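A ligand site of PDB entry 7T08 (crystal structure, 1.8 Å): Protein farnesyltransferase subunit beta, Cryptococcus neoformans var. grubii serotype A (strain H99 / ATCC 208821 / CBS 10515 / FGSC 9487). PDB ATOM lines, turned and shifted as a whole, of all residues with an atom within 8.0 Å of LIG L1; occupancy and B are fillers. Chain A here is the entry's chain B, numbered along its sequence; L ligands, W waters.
Water W2 lies within hydrogen-bond range of the backbone carbonyl oxygen (O) of Gly 488 and a nitrogen (N1) of LIG L1.
Merely in contact with LIG L1: Gly 489 (3.3 Å) and Tyr 58 (3.6 Å).
Within 4 Å of LIG L1: Tyr 58, Gly 489, Lys 490 and Asp 491.
The nearest printed residue that does not touch LIG L1 is Gly 488 (5.3 Å).
OD2 of Asp 491 lies within salt-bridge range of N1 of LIG L1 (2.5 Å).
An oxygen (O3) of LIG L1 lies within hydrogen-bond range of the backbone NH of Asp 491 (3.2 Å).
O2 of LIG L1 is in hydrogen-bond range of N of Lys 490 (2.9 Å).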
ATOM      1  N   LEU A  50      -8.154 -18.749   8.574  1.00  0.00           N
ATOM      2  CA  LEU A  50      -9.126 -19.883   8.522  1.00  0.00           C
ATOM      3  C   LEU A  50      -9.795 -20.163   9.872  1.00  0.00           C
ATOM      4  O   LEU A  50     -10.996 -20.497   9.880  1.00  0.00           O
ATOM      5  CB  LEU A  50      -8.362 -21.107   8.036  1.00  0.00           C
ATOM      6  CG  LEU A  50      -9.134 -22.057   7.132  1.00  0.00           C
ATOM      7  CD1 LEU A  50      -9.260 -21.488   5.730  1.00  0.00           C
ATOM      8  CD2 LEU A  50      -8.467 -23.417   7.092  1.00  0.00           C
ATOM      9  N   TYR A  58     -12.753 -10.438  16.860  1.00  0.00           N
ATOM     10  CA  TYR A  58     -13.254 -10.966  15.596  1.00  0.00           C
ATOM     11  C   TYR A  58     -13.837  -9.822  14.767  1.00  0.00           C
ATOM     12  O   TYR A  58     -14.653  -9.035  15.271  1.00  0.00           O
ATOM     13  CB  TYR A  58     -14.288 -12.057  15.839  1.00  0.00           C
ATOM     14  CG  TYR A  58     -14.855 -12.612  14.548  1.00  0.00           C
ATOM     15  CD1 TYR A  58     -14.019 -13.217  13.619  1.00  0.00           C
ATOM     16  CD2 TYR A  58     -16.202 -12.500  14.244  1.00  0.00           C
ATOM     17  CE1 TYR A  58     -14.502 -13.701  12.428  1.00  0.00           C
ATOM     18  CE2 TYR A  58     -16.705 -12.977  13.049  1.00  0.00           C
ATOM     19  CZ  TYR A  58     -15.847 -13.574  12.143  1.00  0.00           C
ATOM     20  OH  TYR A  58     -16.321 -14.061  10.950  1.00  0.00           O
ATOM     21  N   GLY A  60     -15.750  -9.893  11.952  1.00  0.00           N
ATOM     22  CA  GLY A  60     -16.930 -10.135  11.140  1.00  0.00           C
ATOM     23  C   GLY A  60     -17.900  -8.969  11.141  1.00  0.00           C
ATOM     24  O   GLY A  60     -18.047  -8.276  12.156  1.00  0.00           O
ATOM     25  N   LEU A  61     -18.567  -8.734  10.014  1.00  0.00           N
ATOM     26  CA  LEU A  61     -19.482  -7.618   9.894  1.00  0.00           C
ATOM     27  C   LEU A  61     -20.678  -7.808  10.833  1.00  0.00           C
ATOM     28  O   LEU A  61     -21.413  -8.795  10.711  1.00  0.00           O
ATOM     29  CB  LEU A  61     -19.947  -7.481   8.451  1.00  0.00           C
ATOM     30  CG  LEU A  61     -20.871  -6.274   8.206  1.00  0.00           C
ATOM     31  CD1 LEU A  61     -20.131  -4.934   8.390  1.00  0.00           C
ATOM     32  CD2 LEU A  61     -21.463  -6.376   6.805  1.00  0.00           C
ATOM     33  N   ILE A 486     -15.039 -11.561  -1.183  1.00  0.00           N
ATOM     34  CA  ILE A 486     -15.675 -11.319   0.114  1.00  0.00           C
ATOM     35  C   ILE A 486     -14.632 -11.618   1.190  1.00  0.00           C
ATOM     36  O   ILE A 486     -14.489 -12.766   1.619  1.00  0.00           O
ATOM     37  CB  ILE A 486     -16.952 -12.144   0.326  1.00  0.00           C
ATOM     38  CG1 ILE A 486     -17.883 -12.078  -0.901  1.00  0.00           C
ATOM     39  CG2 ILE A 486     -17.693 -11.621   1.540  1.00  0.00           C
ATOM     40  CD1 ILE A 486     -18.328 -10.628  -1.270  1.00  0.00           C
ATOM     41  N   VAL A 487     -13.937 -10.573   1.660  1.00  0.00           N
ATOM     42  CA  VAL A 487     -12.938 -10.751   2.715  1.00  0.00           C
ATOM     43  C   VAL A 487     -13.627 -11.228   3.990  1.00  0.00           C
ATOM     44  O   VAL A 487     -14.658 -10.682   4.396  1.00  0.00           O
ATOM     45  CB  VAL A 487     -12.179  -9.435   2.960  1.00  0.00           C
ATOM     46  CG1 VAL A 487     -11.301  -9.531   4.208  1.00  0.00           C
ATOM     47  CG2 VAL A 487     -11.334  -9.070   1.729  1.00  0.00           C
ATOM     48  N   GLY A 488     -13.060 -12.266   4.608  1.00  0.00           N
ATOM     49  CA  GLY A 488     -13.560 -12.771   5.872  1.00  0.00           C
ATOM     50  C   GLY A 488     -14.633 -13.839   5.763  1.00  0.00           C
ATOM     51  O   GLY A 488     -15.076 -14.345   6.804  1.00  0.00           O
ATOM     52  N   GLY A 489     -15.067 -14.179   4.559  1.00  0.00           N
ATOM     53  CA  GLY A 489     -16.054 -15.231   4.375  1.00  0.00           C
ATOM     54  C   GLY A 489     -17.408 -14.660   3.975  1.00  0.00           C
ATOM     55  O   GLY A 489     -17.694 -13.472   4.104  1.00  0.00           O
ATOM     56  N   LYS A 490     -18.269 -15.568   3.504  1.00  0.00           N
ATOM     57  CA  LYS A 490     -19.484 -15.152   2.817  1.00  0.00           C
ATOM     58  C   LYS A 490     -20.524 -14.517   3.740  1.00  0.00           C
ATOM     59  O   LYS A 490     -21.375 -13.771   3.247  1.00  0.00           O
ATOM     60  CB  LYS A 490     -20.087 -16.335   2.064  1.00  0.00           C
ATOM     61  CG  LYS A 490     -19.360 -16.623   0.761  1.00  0.00           C
ATOM     62  CD  LYS A 490     -19.912 -17.863   0.072  1.00  0.00           C
ATOM     63  CE  LYS A 490     -19.080 -18.224  -1.152  1.00  0.00           C
ATOM     64  NZ  LYS A 490     -19.346 -19.619  -1.605  1.00  0.00           N
ATOM     65  N   ASP A 491     -20.447 -14.751   5.054  1.00  0.00           N
ATOM     66  CA  ASP A 491     -21.342 -14.024   5.946  1.00  0.00           C
ATOM     67  C   ASP A 491     -21.064 -12.520   5.976  1.00  0.00           C
ATOM     68  O   ASP A 491     -21.917 -11.764   6.476  1.00  0.00           O
ATOM     69  CB  ASP A 491     -21.267 -14.592   7.366  1.00  0.00           C
ATOM     70  CG  ASP A 491     -21.948 -15.954   7.485  1.00  0.00           C
ATOM     71  OD1 ASP A 491     -23.020 -16.133   6.862  1.00  0.00           O
ATOM     72  OD2 ASP A 491     -21.411 -16.838   8.191  1.00  0.00           O
ATOM     73  N   ASN A 492     -19.920 -12.058   5.481  1.00  0.00           N
ATOM     74  CA  ASN A 492     -19.679 -10.627   5.383  1.00  0.00           C
ATOM     75  C   ASN A 492     -20.264 -10.009   4.117  1.00  0.00           C
ATOM     76  O   ASN A 492     -20.179  -8.788   3.960  1.00  0.00           O
ATOM     77  CB  ASN A 492     -18.172 -10.312   5.440  1.00  0.00           C
ATOM     78  CG  ASN A 492     -17.591 -10.529   6.819  1.00  0.00           C
ATOM     79  OD1 ASN A 492     -18.311 -10.559   7.826  1.00  0.00           O
ATOM     80  ND2 ASN A 492     -16.271 -10.691   6.883  1.00  0.00           N
ATOM     81  N   ARG A 493     -20.835 -10.791   3.218  1.00  0.00           N
ATOM     82  CA  ARG A 493     -21.300 -10.252   1.940  1.00  0.00           C
ATOM     83  C   ARG A 493     -22.489  -9.329   2.133  1.00  0.00           C
ATOM     84  O   ARG A 493     -23.435  -9.653   2.861  1.00  0.00           O
ATOM     85  CB  ARG A 493     -21.684 -11.391   0.986  1.00  0.00           C
ATOM     86  CG  ARG A 493     -22.146 -10.879  -0.396  1.00  0.00           C
ATOM     87  CD  ARG A 493     -23.188 -11.804  -1.025  1.00  0.00           C
ATOM     88  NE  ARG A 493     -23.589 -11.367  -2.356  1.00  0.00           N
ATOM     89  CZ  ARG A 493     -24.715 -10.696  -2.636  1.00  0.00           C
ATOM     90  NH1 ARG A 493     -25.570 -10.369  -1.667  1.00  0.00           N
ATOM     91  NH2 ARG A 493     -24.985 -10.353  -3.884  1.00  0.00           N
HETATM   92  O1  LIG L   1     -17.134 -20.601   3.336  1.00  0.00           O
HETATM   93  O2  LIG L   1     -17.087 -18.261   3.442  1.00  0.00           O
HETATM   94  O3  LIG L   1     -19.339 -17.609   5.925  1.00  0.00           O
HETATM   95  O4  LIG L   1     -19.301 -19.424   3.376  1.00  0.00           O
HETATM   96  C1  LIG L   1     -19.907 -17.570  12.787  1.00  0.00           C
HETATM   97  C2  LIG L   1     -19.388 -18.845  12.127  1.00  0.00           C
HETATM   98  C3  LIG L   1     -19.187 -16.311  12.272  1.00  0.00           C
HETATM   99  C4  LIG L   1     -19.394 -18.759  10.591  1.00  0.00           C
HETATM  100  C5  LIG L   1     -19.231 -16.218  10.749  1.00  0.00           C
HETATM  101  C6  LIG L   1     -18.229 -18.412   7.924  1.00  0.00           C
HETATM  102  C7  LIG L   1     -17.773 -19.525   5.729  1.00  0.00           C
HETATM  103  N1  LIG L   1     -18.996 -17.387   8.618  1.00  0.00           N
HETATM  104  C8  LIG L   1     -18.816 -18.750   6.550  1.00  0.00           C
HETATM  105  C9  LIG L   1     -18.719 -17.488  10.059  1.00  0.00           C
HETATM  106  S1  LIG L   1     -17.891 -19.432   3.923  1.00  0.00           S
HETATM  107  O1  LG2 L   2     -22.632  -9.003  16.115  1.00  0.00           O
HETATM  108  O2  LG2 L   2     -24.380  -8.076  14.637  1.00  0.00           O
HETATM  109  O3  LG2 L   2     -23.605 -10.412  18.190  1.00  0.00           O
HETATM  110  O4  LG2 L   2     -23.885 -10.355  14.395  1.00  0.00           O
HETATM  111  C1  LG2 L   2     -26.396 -15.078  21.765  1.00  0.00           C
HETATM  112  C2  LG2 L   2     -26.396 -13.773  22.558  1.00  0.00           C
HETATM  113  C3  LG2 L   2     -27.048 -14.899  20.394  1.00  0.00           C
HETATM  114  C4  LG2 L   2     -25.711 -12.644  21.782  1.00  0.00           C
HETATM  115  C5  LG2 L   2     -26.326 -13.822  19.591  1.00  0.00           C
HETATM  116  C6  LG2 L   2     -25.901 -10.648  18.821  1.00  0.00           C
HETATM  117  C7  LG2 L   2     -25.290  -9.648  16.635  1.00  0.00           C
HETATM  118  N1  LG2 L   2     -25.235 -11.664  19.626  1.00  0.00           N
HETATM  119  C8  LG2 L   2     -24.858  -9.791  18.090  1.00  0.00           C
HETATM  120  C9  LG2 L   2     -26.206 -12.497  20.338  1.00  0.00           C
HETATM  121  S1  LG2 L   2     -23.960  -9.265  15.443  1.00  0.00           S
HETATM  122  O   HOH W   1     -16.098 -23.021   4.756  1.00  0.00           O
HETATM  123  O   HOH W   2     -17.810 -14.958   7.518  1.00  0.00           O
HETATM  124  O   HOH W   3     -15.170 -17.749   7.580  1.00  0.00           O
